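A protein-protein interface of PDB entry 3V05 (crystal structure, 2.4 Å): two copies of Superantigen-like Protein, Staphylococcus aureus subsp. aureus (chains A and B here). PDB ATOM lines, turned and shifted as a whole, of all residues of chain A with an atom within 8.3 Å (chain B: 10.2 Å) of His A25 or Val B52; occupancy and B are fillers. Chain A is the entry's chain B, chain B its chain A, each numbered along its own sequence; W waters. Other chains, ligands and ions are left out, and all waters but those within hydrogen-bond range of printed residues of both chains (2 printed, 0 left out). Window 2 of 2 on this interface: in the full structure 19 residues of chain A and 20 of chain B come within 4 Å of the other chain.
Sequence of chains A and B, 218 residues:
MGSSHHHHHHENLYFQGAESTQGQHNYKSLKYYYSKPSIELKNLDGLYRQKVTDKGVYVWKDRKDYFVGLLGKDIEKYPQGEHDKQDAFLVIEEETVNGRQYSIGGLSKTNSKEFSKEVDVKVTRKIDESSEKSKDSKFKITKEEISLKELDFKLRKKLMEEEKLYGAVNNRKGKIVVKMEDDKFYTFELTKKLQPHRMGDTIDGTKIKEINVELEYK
The backbone NH (N) of Lys B51 sits at hydrogen-bond distance from the side-chain carboxylate (OD2) of Asp B54 (2.9 Å).
A ring nitrogen (ND1) of His A25 lies within hydrogen-bond range of the backbone NH of Tyr A27 (3.2 Å).
The backbone carbonyl oxygen (O) of Asn A26 sits at hydrogen-bond distance from the side-chain hydroxyl (OG) of Ser A29, at 3.0 Å.
The guanidinium group of Arg B49 is in hydrogen-bond range of the backbone carbonyl oxygen of Val B52 (3.4 Å).
The guanidinium group of Arg B49 is in hydrogen-bond range of the backbone carbonyl oxygen of Lys B51, 3.2 Å away.
The backbone carbonyl oxygen (O) of Lys B55 is in hydrogen-bond range of the backbone NH (N) of Leu B70.
No position is printed for both chains.
Of the 7 pairs that touch across the chains among the printed residues, none has its exchanged pair printed and touching as well.
Hydrophobic or aromatic side chains of chain B that line the printed part of chain A: Val B52.
Of the 15 printed residues of chain A, 5 touch a printed residue of chain B.
Hydrophobic or aromatic side chains of chain A that line the printed part of chain B: Tyr A32 and Tyr A33.
Along chain A the printed residues that touch a printed residue of chain B span positions 25 to 94.
No residue of chain B comes within 4 Å of Asn A26.
No residue of chain B comes within 4 Å of Lys A28.
Ser A29 touches just one residue of chain B: Val B52.
Printed residues of chain A within 4 Å of Lys B51: Glu A94 (3.0 Å).
Of the printed residues of chain A, Thr B53 touches Tyr A32 (3.6 Å) and Glu A94 (3.5 Å).
Printed residues of chain B within 4 Å of Tyr A32: Thr B53.
Of the printed residues of chain B, Tyr A33 touches Lys B55 (3.6 Å).
Printed residues of chain A within 4 Å of Asp B54: Glu A94.
Val B57 touches none of the printed residues of chain A.
The nearest printed residue of chain A that does not touch Lys B55 is Lys A193 (4.3 Å).
The side-chain carboxylate of Glu A94 is in salt-bridge range of the side-chain amino group of Lys B51 (3.0 Å).
Water W2 lies within hydrogen-bond range of the backbone carbonyl oxygen of Asp B54 (3.0 Å), the backbone carbonyl oxygen of Thr B53 (3.1 Å), the side-chain amino group of Lys A193 (3.3 Å) and the side-chain amino group of Lys B55 (3.4 Å).
Water W1 bridges N of Glu A94 (3.1 Å) and N of Lys B55 (3.3 Å).
Among the printed residues, merely in contact across the chains: Ser A29 with Val B52, Glu A94 with Thr B53, Tyr A33 with Lys B55, Tyr A32 with Thr B53, His A25 with Val B52 and Glu A94 with Asp B54.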
ATOM      1  N   HIS A  25       2.818 -24.089  10.755  1.00  0.00           N
ATOM      2  CA  HIS A  25       3.599 -22.894  10.323  1.00  0.00           C
ATOM      3  C   HIS A  25       4.779 -22.730  11.284  1.00  0.00           C
ATOM      4  O   HIS A  25       4.802 -23.326  12.371  1.00  0.00           O
ATOM      5  CB  HIS A  25       2.704 -21.643  10.332  1.00  0.00           C
ATOM      6  CG  HIS A  25       3.241 -20.491   9.530  1.00  0.00           C
ATOM      7  ND1 HIS A  25       4.126 -19.566  10.044  1.00  0.00           N
ATOM      8  CD2 HIS A  25       2.997 -20.107   8.254  1.00  0.00           C
ATOM      9  CE1 HIS A  25       4.414 -18.671   9.116  1.00  0.00           C
ATOM     10  NE2 HIS A  25       3.742 -18.975   8.021  1.00  0.00           N
ATOM     11  N   ASN A  26       5.766 -21.939  10.868  1.00  0.00           N
ATOM     12  CA  ASN A  26       6.945 -21.677  11.685  1.00  0.00           C
ATOM     13  C   ASN A  26       6.572 -20.924  12.961  1.00  0.00           C
ATOM     14  O   ASN A  26       7.134 -21.173  14.019  1.00  0.00           O
ATOM     15  CB  ASN A  26       7.965 -20.870  10.881  1.00  0.00           C
ATOM     16  CG  ASN A  26       9.289 -20.712  11.602  1.00  0.00           C
ATOM     17  OD1 ASN A  26       9.769 -21.641  12.262  1.00  0.00           O
ATOM     18  ND2 ASN A  26       9.903 -19.538  11.456  1.00  0.00           N
ATOM     19  N   TYR A  27       5.617 -20.006  12.843  1.00  0.00           N
ATOM     20  CA  TYR A  27       5.128 -19.204  13.970  1.00  0.00           C
ATOM     21  C   TYR A  27       4.514 -20.049  15.093  1.00  0.00           C
ATOM     22  O   TYR A  27       4.858 -19.877  16.268  1.00  0.00           O
ATOM     23  CB  TYR A  27       4.111 -18.175  13.460  1.00  0.00           C
ATOM     24  CG  TYR A  27       3.249 -17.526  14.525  1.00  0.00           C
ATOM     25  CD1 TYR A  27       1.893 -17.846  14.642  1.00  0.00           C
ATOM     26  CD2 TYR A  27       3.779 -16.596  15.418  1.00  0.00           C
ATOM     27  CE1 TYR A  27       1.087 -17.249  15.613  1.00  0.00           C
ATOM     28  CE2 TYR A  27       2.981 -15.995  16.393  1.00  0.00           C
ATOM     29  CZ  TYR A  27       1.638 -16.325  16.488  1.00  0.00           C
ATOM     30  OH  TYR A  27       0.844 -15.738  17.452  1.00  0.00           O
ATOM     31  N   LYS A  28       3.610 -20.957  14.730  1.00  0.00           N
ATOM     32  CA  LYS A  28       2.952 -21.804  15.722  1.00  0.00           C
ATOM     33  C   LYS A  28       3.936 -22.682  16.492  1.00  0.00           C
ATOM     34  O   LYS A  28       3.813 -22.820  17.705  1.00  0.00           O
ATOM     35  CB  LYS A  28       1.865 -22.670  15.075  1.00  0.00           C
ATOM     36  CG  LYS A  28       0.680 -21.872  14.560  1.00  0.00           C
ATOM     37  CD  LYS A  28      -0.378 -22.755  13.882  1.00  0.00           C
ATOM     38  CE  LYS A  28      -1.010 -23.752  14.856  1.00  0.00           C
ATOM     39  NZ  LYS A  28      -2.086 -24.548  14.206  1.00  0.00           N
ATOM     40  N   SER A  29       4.912 -23.264  15.796  1.00  0.00           N
ATOM     41  CA  SER A  29       5.900 -24.123  16.458  1.00  0.00           C
ATOM     42  C   SER A  29       6.814 -23.347  17.419  1.00  0.00           C
ATOM     43  O   SER A  29       7.260 -23.904  18.413  1.00  0.00           O
ATOM     44  CB  SER A  29       6.728 -24.924  15.443  1.00  0.00           C
ATOM     45  OG  SER A  29       7.427 -24.090  14.544  1.00  0.00           O
ATOM     46  N   LEU A  30       7.094 -22.075  17.123  1.00  0.00           N
ATOM     47  CA  LEU A  30       7.920 -21.237  18.010  1.00  0.00           C
ATOM     48  C   LEU A  30       7.123 -20.836  19.250  1.00  0.00           C
ATOM     49  O   LEU A  30       7.556 -21.042  20.391  1.00  0.00           O
ATOM     50  CB  LEU A  30       8.390 -19.980  17.282  1.00  0.00           C
ATOM     51  CG  LEU A  30       9.406 -20.183  16.160  1.00  0.00           C
ATOM     52  CD1 LEU A  30       9.510 -18.933  15.299  1.00  0.00           C
ATOM     53  CD2 LEU A  30      10.757 -20.591  16.734  1.00  0.00           C
ATOM     54  N   LYS A  31       5.956 -20.258  18.993  1.00  0.00           N
ATOM     55  CA  LYS A  31       5.024 -19.798  20.021  1.00  0.00           C
ATOM     56  C   LYS A  31       4.647 -20.888  21.037  1.00  0.00           C
ATOM     57  O   LYS A  31       4.727 -20.668  22.245  1.00  0.00           O
ATOM     58  CB  LYS A  31       3.764 -19.270  19.309  1.00  0.00           C
ATOM     59  CG  LYS A  31       2.569 -18.854  20.169  1.00  0.00           C
ATOM     60  CD  LYS A  31       2.879 -17.706  21.096  1.00  0.00           C
ATOM     61  CE  LYS A  31       1.587 -16.964  21.490  1.00  0.00           C
ATOM     62  NZ  LYS A  31       1.841 -15.784  22.381  1.00  0.00           N
ATOM     63  N   TYR A  32       4.257 -22.062  20.549  1.00  0.00           N
ATOM     64  CA  TYR A  32       3.822 -23.141  21.448  1.00  0.00           C
ATOM     65  C   TYR A  32       4.955 -23.961  22.048  1.00  0.00           C
ATOM     66  O   TYR A  32       4.715 -24.819  22.901  1.00  0.00           O
ATOM     67  CB  TYR A  32       2.765 -24.025  20.774  1.00  0.00           C
ATOM     68  CG  TYR A  32       1.566 -23.212  20.325  1.00  0.00           C
ATOM     69  CD1 TYR A  32       0.851 -22.439  21.241  1.00  0.00           C
ATOM     70  CD2 TYR A  32       1.140 -23.217  18.999  1.00  0.00           C
ATOM     71  CE1 TYR A  32      -0.238 -21.681  20.849  1.00  0.00           C
ATOM     72  CE2 TYR A  32       0.041 -22.461  18.597  1.00  0.00           C
ATOM     73  CZ  TYR A  32      -0.643 -21.696  19.529  1.00  0.00           C
ATOM     74  OH  TYR A  32      -1.734 -20.942  19.155  1.00  0.00           O
ATOM     75  N   TYR A  33       6.188 -23.706  21.617  1.00  0.00           N
ATOM     76  CA  TYR A  33       7.326 -24.377  22.206  1.00  0.00           C
ATOM     77  C   TYR A  33       7.856 -23.519  23.345  1.00  0.00           C
ATOM     78  O   TYR A  33       7.986 -23.984  24.479  1.00  0.00           O
ATOM     79  CB  TYR A  33       8.442 -24.634  21.189  1.00  0.00           C
ATOM     80  CG  TYR A  33       9.582 -25.413  21.807  1.00  0.00           C
ATOM     81  CD1 TYR A  33      10.721 -24.767  22.283  1.00  0.00           C
ATOM     82  CD2 TYR A  33       9.494 -26.796  21.966  1.00  0.00           C
ATOM     83  CE1 TYR A  33      11.766 -25.483  22.872  1.00  0.00           C
ATOM     84  CE2 TYR A  33      10.532 -27.525  22.564  1.00  0.00           C
ATOM     85  CZ  TYR A  33      11.664 -26.861  23.016  1.00  0.00           C
ATOM     86  OH  TYR A  33      12.697 -27.578  23.589  1.00  0.00           O
ATOM     87  N   GLU A  94       7.076 -33.259  23.571  1.00  0.00           N
ATOM     88  CA  GLU A  94       5.840 -33.971  23.258  1.00  0.00           C
ATOM     89  C   GLU A  94       5.969 -35.484  23.323  1.00  0.00           C
ATOM     90  O   GLU A  94       4.995 -36.184  23.627  1.00  0.00           O
ATOM     91  CB  GLU A  94       5.346 -33.571  21.857  1.00  0.00           C
ATOM     92  CG  GLU A  94       4.975 -32.111  21.765  1.00  0.00           C
ATOM     93  CD  GLU A  94       3.826 -31.777  22.687  1.00  0.00           C
ATOM     94  OE1 GLU A  94       3.937 -30.804  23.452  1.00  0.00           O
ATOM     95  OE2 GLU A  94       2.821 -32.512  22.669  1.00  0.00           O
ATOM     96  N   VAL A 169       1.919 -13.308  14.204  1.00  0.00           N
ATOM     97  CA  VAL A 169       2.627 -13.941  13.082  1.00  0.00           C
ATOM     98  C   VAL A 169       3.866 -13.170  12.608  1.00  0.00           C
ATOM     99  O   VAL A 169       4.863 -13.777  12.202  1.00  0.00           O
ATOM    100  CB  VAL A 169       1.659 -14.179  11.881  1.00  0.00           C
ATOM    101  CG1 VAL A 169       2.420 -14.548  10.614  1.00  0.00           C
ATOM    102  CG2 VAL A 169       0.643 -15.257  12.226  1.00  0.00           C
ATOM    103  N   ASN A 170       3.796 -11.843  12.686  1.00  0.00           N
ATOM    104  CA  ASN A 170       4.872 -10.961  12.241  1.00  0.00           C
ATOM    105  C   ASN A 170       6.004 -10.751  13.275  1.00  0.00           C
ATOM    106  O   ASN A 170       7.054 -10.205  12.931  1.00  0.00           O
ATOM    107  CB  ASN A 170       4.249  -9.604  11.859  1.00  0.00           C
ATOM    108  CG  ASN A 170       5.165  -8.737  10.997  1.00  0.00           C
ATOM    109  OD1 ASN A 170       6.196  -9.191  10.497  1.00  0.00           O
ATOM    110  ND2 ASN A 170       4.773  -7.482  10.806  1.00  0.00           N
ATOM    111  N   ARG A 172       8.572 -12.509  14.875  1.00  0.00           N
ATOM    112  CA  ARG A 172       9.496 -13.647  14.983  1.00  0.00           C
ATOM    113  C   ARG A 172      10.938 -13.414  14.500  1.00  0.00           C
ATOM    114  O   ARG A 172      11.797 -14.270  14.714  1.00  0.00           O
ATOM    115  CB  ARG A 172       8.896 -14.856  14.249  1.00  0.00           C
ATOM    116  CG  ARG A 172       8.245 -14.522  12.924  1.00  0.00           C
ATOM    117  CD  ARG A 172       7.776 -15.766  12.174  1.00  0.00           C
ATOM    118  NE  ARG A 172       8.864 -16.414  11.439  1.00  0.00           N
ATOM    119  CZ  ARG A 172       9.238 -16.078  10.199  1.00  0.00           C
ATOM    120  NH1 ARG A 172       8.628 -15.088   9.546  1.00  0.00           N
ATOM    121  NH2 ARG A 172      10.239 -16.724   9.605  1.00  0.00           N
ATOM    122  N   THR A 191      13.949 -16.785  14.540  1.00  0.00           N
ATOM    123  CA  THR A 191      13.046 -17.348  13.525  1.00  0.00           C
ATOM    124  C   THR A 191      12.946 -18.869  13.578  1.00  0.00           C
ATOM    125  O   THR A 191      12.122 -19.444  12.899  1.00  0.00           O
ATOM    126  CB  THR A 191      13.420 -16.921  12.096  1.00  0.00           C
ATOM    127  OG1 THR A 191      14.768 -17.308  11.815  1.00  0.00           O
ATOM    128  CG2 THR A 191      13.263 -15.406  11.930  1.00  0.00           C
ATOM    129  N   LYS A 193      13.664 -22.602  16.291  1.00  0.00           N
ATOM    130  CA  LYS A 193      13.980 -23.138  17.607  1.00  0.00           C
ATOM    131  C   LYS A 193      15.464 -23.487  17.718  1.00  0.00           C
ATOM    132  O   LYS A 193      16.104 -23.827  16.722  1.00  0.00           O
ATOM    133  CB  LYS A 193      13.135 -24.380  17.902  1.00  0.00           C
ATOM    134  CG  LYS A 193      11.628 -24.141  17.835  1.00  0.00           C
ATOM    135  CD  LYS A 193      10.809 -25.284  18.460  1.00  0.00           C
ATOM    136  CE  LYS A 193      11.033 -26.621  17.804  1.00  0.00           C
ATOM    137  NZ  LYS A 193      10.628 -26.674  16.369  1.00  0.00           N
ATOM    138  N   TYR B  48       3.234 -39.613   9.034  1.00  0.00           N
ATOM    139  CA  TYR B  48       2.369 -38.594   9.624  1.00  0.00           C
ATOM    140  C   TYR B  48       3.018 -37.785  10.741  1.00  0.00           C
ATOM    141  O   TYR B  48       3.541 -38.346  11.706  1.00  0.00           O
ATOM    142  CB  TYR B  48       1.102 -39.293  10.139  1.00  0.00           C
ATOM    143  CG  TYR B  48       0.112 -38.422  10.887  1.00  0.00           C
ATOM    144  CD1 TYR B  48      -0.558 -37.389  10.248  1.00  0.00           C
ATOM    145  CD2 TYR B  48      -0.193 -38.672  12.221  1.00  0.00           C
ATOM    146  CE1 TYR B  48      -1.481 -36.603  10.920  1.00  0.00           C
ATOM    147  CE2 TYR B  48      -1.116 -37.885  12.905  1.00  0.00           C
ATOM    148  CZ  TYR B  48      -1.753 -36.855  12.245  1.00  0.00           C
ATOM    149  OH  TYR B  48      -2.668 -36.078  12.905  1.00  0.00           O
ATOM    150  N   ARG B  49       2.979 -36.462  10.589  1.00  0.00           N
ATOM    151  CA  ARG B  49       3.499 -35.536  11.587  1.00  0.00           C
ATOM    152  C   ARG B  49       2.283 -35.119  12.403  1.00  0.00           C
ATOM    153  O   ARG B  49       1.405 -34.420  11.899  1.00  0.00           O
ATOM    154  CB  ARG B  49       4.144 -34.324  10.918  1.00  0.00           C
ATOM    155  CG  ARG B  49       4.746 -33.291  11.875  1.00  0.00           C
ATOM    156  CD  ARG B  49       6.129 -33.692  12.395  1.00  0.00           C
ATOM    157  NE  ARG B  49       6.617 -32.735  13.383  1.00  0.00           N
ATOM    158  CZ  ARG B  49       7.170 -31.551  13.100  1.00  0.00           C
ATOM    159  NH1 ARG B  49       7.313 -31.144  11.840  1.00  0.00           N
ATOM    160  NH2 ARG B  49       7.575 -30.759  14.091  1.00  0.00           N
ATOM    161  N   GLN B  50       2.235 -35.547  13.663  1.00  0.00           N
ATOM    162  CA  GLN B  50       1.087 -35.280  14.528  1.00  0.00           C
ATOM    163  C   GLN B  50       0.950 -33.818  14.958  1.00  0.00           C
ATOM    164  O   GLN B  50      -0.095 -33.202  14.753  1.00  0.00           O
ATOM    165  CB  GLN B  50       1.146 -36.178  15.769  1.00  0.00           C
ATOM    166  CG  GLN B  50      -0.121 -36.136  16.629  1.00  0.00           C
ATOM    167  CD  GLN B  50      -0.052 -37.056  17.837  1.00  0.00           C
ATOM    168  OE1 GLN B  50       1.033 -37.375  18.341  1.00  0.00           O
ATOM    169  NE2 GLN B  50      -1.216 -37.488  18.310  1.00  0.00           N
ATOM    170  N   LYS B  51       2.010 -33.273  15.545  1.00  0.00           N
ATOM    171  CA  LYS B  51       1.989 -31.906  16.050  1.00  0.00           C
ATOM    172  C   LYS B  51       3.164 -31.104  15.539  1.00  0.00           C
ATOM    173  O   LYS B  51       4.253 -31.638  15.316  1.00  0.00           O
ATOM    174  CB  LYS B  51       2.034 -31.913  17.582  1.00  0.00           C
ATOM    175  CG  LYS B  51       0.948 -32.743  18.247  1.00  0.00           C
ATOM    176  CD  LYS B  51       1.095 -32.718  19.764  1.00  0.00           C
ATOM    177  CE  LYS B  51       0.040 -33.587  20.447  1.00  0.00           C
ATOM    178  NZ  LYS B  51       0.113 -33.526  21.935  1.00  0.00           N
ATOM    179  N   VAL B  52       2.941 -29.806  15.376  1.00  0.00           N
ATOM    180  CA  VAL B  52       3.974 -28.901  14.909  1.00  0.00           C
ATOM    181  C   VAL B  52       4.983 -28.683  16.044  1.00  0.00           C
ATOM    182  O   VAL B  52       6.096 -28.208  15.820  1.00  0.00           O
ATOM    183  CB  VAL B  52       3.365 -27.551  14.454  1.00  0.00           C
ATOM    184  CG1 VAL B  52       2.818 -26.774  15.653  1.00  0.00           C
ATOM    185  CG2 VAL B  52       4.397 -26.723  13.699  1.00  0.00           C
ATOM    186  N   THR B  53       4.569 -29.037  17.260  1.00  0.00           N
ATOM    187  CA  THR B  53       5.396 -28.929  18.451  1.00  0.00           C
ATOM    188  C   THR B  53       6.258 -30.169  18.725  1.00  0.00           C
ATOM    189  O   THR B  53       7.238 -30.075  19.469  1.00  0.00           O
ATOM    190  CB  THR B  53       4.528 -28.684  19.693  1.00  0.00           C
ATOM    191  OG1 THR B  53       3.464 -29.646  19.727  1.00  0.00           O
ATOM    192  CG2 THR B  53       3.942 -27.267  19.674  1.00  0.00           C
ATOM    193  N   ASP B  54       5.905 -31.315  18.137  1.00  0.00           N
ATOM    194  CA  ASP B  54       6.665 -32.553  18.363  1.00  0.00           C
ATOM    195  C   ASP B  54       7.944 -32.620  17.504  1.00  0.00           C
ATOM    196  O   ASP B  54       8.177 -31.765  16.651  1.00  0.00           O
ATOM    197  CB  ASP B  54       5.776 -33.803  18.167  1.00  0.00           C
ATOM    198  CG  ASP B  54       5.424 -34.067  16.715  1.00  0.00           C
ATOM    199  OD1 ASP B  54       6.212 -33.687  15.831  1.00  0.00           O
ATOM    200  OD2 ASP B  54       4.361 -34.682  16.463  1.00  0.00           O
ATOM    201  N   LYS B  55       8.763 -33.639  17.746  1.00  0.00           N
ATOM    202  CA  LYS B  55      10.037 -33.818  17.043  1.00  0.00           C
ATOM    203  C   LYS B  55      10.138 -35.151  16.288  1.00  0.00           C
ATOM    204  O   LYS B  55      11.149 -35.851  16.365  1.00  0.00           O
ATOM    205  CB  LYS B  55      11.208 -33.682  18.037  1.00  0.00           C
ATOM    206  CG  LYS B  55      11.474 -32.249  18.514  1.00  0.00           C
ATOM    207  CD  LYS B  55      12.669 -32.188  19.455  1.00  0.00           C
ATOM    208  CE  LYS B  55      13.085 -30.750  19.779  1.00  0.00           C
ATOM    209  NZ  LYS B  55      12.005 -29.934  20.408  1.00  0.00           N
ATOM    210  N   GLY B  56       9.096 -35.509  15.554  1.00  0.00           N
ATOM    211  CA  GLY B  56       9.136 -36.745  14.786  1.00  0.00           C
ATOM    212  C   GLY B  56       7.864 -37.058  14.039  1.00  0.00           C
ATOM    213  O   GLY B  56       6.884 -36.321  14.127  1.00  0.00           O
ATOM    214  N   VAL B  57       7.891 -38.170  13.311  1.00  0.00           N
ATOM    215  CA  VAL B  57       6.745 -38.630  12.534  1.00  0.00           C
ATOM    216  C   VAL B  57       6.514 -40.133  12.688  1.00  0.00           C
ATOM    217  O   VAL B  57       7.466 -40.917  12.867  1.00  0.00           O
ATOM    218  CB  VAL B  57       6.917 -38.315  11.026  1.00  0.00           C
ATOM    219  CG1 VAL B  57       6.814 -36.828  10.767  1.00  0.00           C
ATOM    220  CG2 VAL B  57       8.227 -38.865  10.503  1.00  0.00           C
ATOM    221  N   LEU B  70      12.967 -36.405  14.159  1.00  0.00           N
ATOM    222  CA  LEU B  70      13.444 -35.374  13.238  1.00  0.00           C
ATOM    223  C   LEU B  70      14.261 -34.400  14.080  1.00  0.00           C
ATOM    224  O   LEU B  70      13.720 -33.436  14.622  1.00  0.00           O
ATOM    225  CB  LEU B  70      12.259 -34.682  12.568  1.00  0.00           C
ATOM    226  CG  LEU B  70      11.375 -35.560  11.673  1.00  0.00           C
ATOM    227  CD1 LEU B  70      10.116 -34.822  11.255  1.00  0.00           C
ATOM    228  CD2 LEU B  70      12.137 -36.052  10.434  1.00  0.00           C
ATOM    229  N   ILE B  75      13.507 -31.825   9.937  1.00  0.00           N
ATOM    230  CA  ILE B  75      12.227 -31.483  10.558  1.00  0.00           C
ATOM    231  C   ILE B  75      11.424 -30.492   9.703  1.00  0.00           C
ATOM    232  O   ILE B  75      10.196 -30.546   9.676  1.00  0.00           O
ATOM    233  CB  ILE B  75      12.416 -30.908  11.981  1.00  0.00           C
ATOM    234  CG1 ILE B  75      11.076 -30.862  12.723  1.00  0.00           C
ATOM    235  CG2 ILE B  75      13.075 -29.520  11.937  1.00  0.00           C
ATOM    236  CD1 ILE B  75      11.193 -30.431  14.163  1.00  0.00           C
ATOM    237  N   GLU B  76      12.126 -29.613   8.990  1.00  0.00           N
ATOM    238  CA  GLU B  76      11.489 -28.606   8.127  1.00  0.00           C
ATOM    239  C   GLU B  76      10.780 -29.186   6.887  1.00  0.00           C
ATOM    240  O   GLU B  76       9.927 -28.524   6.288  1.00  0.00           O
ATOM    241  CB  GLU B  76      12.533 -27.565   7.697  1.00  0.00           C
ATOM    242  CG  GLU B  76      13.110 -26.757   8.870  1.00  0.00           C
ATOM    243  CD  GLU B  76      14.241 -25.822   8.463  1.00  0.00           C
ATOM    244  OE1 GLU B  76      14.646 -25.835   7.279  1.00  0.00           O
ATOM    245  OE2 GLU B  76      14.732 -25.074   9.337  1.00  0.00           O
ATOM    246  N   TYR B  78       8.896 -31.939   6.943  1.00  0.00           N
ATOM    247  CA  TYR B  78       7.678 -32.647   7.332  1.00  0.00           C
ATOM    248  C   TYR B  78       6.767 -31.857   8.266  1.00  0.00           C
ATOM    249  O   TYR B  78       6.676 -32.152   9.452  1.00  0.00           O
ATOM    250  CB  TYR B  78       8.051 -34.006   7.942  1.00  0.00           C
ATOM    251  CG  TYR B  78       8.906 -34.827   6.998  1.00  0.00           C
ATOM    252  CD1 TYR B  78       8.345 -35.437   5.881  1.00  0.00           C
ATOM    253  CD2 TYR B  78      10.277 -34.970   7.209  1.00  0.00           C
ATOM    254  CE1 TYR B  78       9.121 -36.175   5.002  1.00  0.00           C
ATOM    255  CE2 TYR B  78      11.066 -35.714   6.340  1.00  0.00           C
ATOM    256  CZ  TYR B  78      10.480 -36.313   5.236  1.00  0.00           C
ATOM    257  OH  TYR B  78      11.241 -37.044   4.361  1.00  0.00           O
ATOM    258  N   PRO B  79       6.081 -30.844   7.725  1.00  0.00           N
ATOM    259  CA  PRO B  79       5.134 -30.099   8.545  1.00  0.00           C
ATOM    260  C   PRO B  79       3.929 -30.972   8.913  1.00  0.00           C
ATOM    261  O   PRO B  79       3.725 -32.039   8.312  1.00  0.00           O
ATOM    262  CB  PRO B  79       4.720 -28.945   7.637  1.00  0.00           C
ATOM    263  CG  PRO B  79       4.966 -29.441   6.254  1.00  0.00           C
ATOM    264  CD  PRO B  79       6.177 -30.296   6.360  1.00  0.00           C
ATOM    265  N   GLN B  80       3.145 -30.515   9.887  1.00  0.00           N
ATOM    266  CA  GLN B  80       1.979 -31.261  10.387  1.00  0.00           C
ATOM    267  C   GLN B  80       1.134 -31.810   9.239  1.00  0.00           C
ATOM    268  O   GLN B  80       0.900 -31.129   8.252  1.00  0.00           O
ATOM    269  CB  GLN B  80       1.128 -30.368  11.310  1.00  0.00           C
ATOM    270  CG  GLN B  80       0.133 -31.109  12.202  1.00  0.00           C
ATOM    271  CD  GLN B  80      -1.046 -31.692  11.454  1.00  0.00           C
ATOM    272  OE1 GLN B  80      -1.552 -31.092  10.507  1.00  0.00           O
ATOM    273  NE2 GLN B  80      -1.507 -32.866  11.893  1.00  0.00           N
ATOM    274  N   GLY B  81       0.686 -33.053   9.381  1.00  0.00           N
ATOM    275  CA  GLY B  81      -0.141 -33.705   8.367  1.00  0.00           C
ATOM    276  C   GLY B  81       0.529 -34.958   7.837  1.00  0.00           C
ATOM    277  O   GLY B  81       1.515 -35.434   8.414  1.00  0.00           O
ATOM    278  N   HIS B  83       2.300 -37.310   4.590  1.00  0.00           N
ATOM    279  CA  HIS B  83       3.200 -37.172   3.457  1.00  0.00           C
ATOM    280  C   HIS B  83       3.346 -38.530   2.820  1.00  0.00           C
ATOM    281  O   HIS B  83       3.306 -39.542   3.517  1.00  0.00           O
ATOM    282  CB  HIS B  83       4.569 -36.665   3.936  1.00  0.00           C
ATOM    283  CG  HIS B  83       4.484 -35.435   4.784  1.00  0.00           C
ATOM    284  ND1 HIS B  83       4.478 -34.162   4.253  1.00  0.00           N
ATOM    285  CD2 HIS B  83       4.372 -35.284   6.126  1.00  0.00           C
ATOM    286  CE1 HIS B  83       4.369 -33.281   5.231  1.00  0.00           C
ATOM    287  NE2 HIS B  83       4.306 -33.935   6.376  1.00  0.00           N
HETATM  288  O   HOH W   1       8.768 -32.904  20.997  1.00  0.00           O
HETATM  289  O   HOH W   2       9.857 -29.549  17.804  1.00  0.00           O
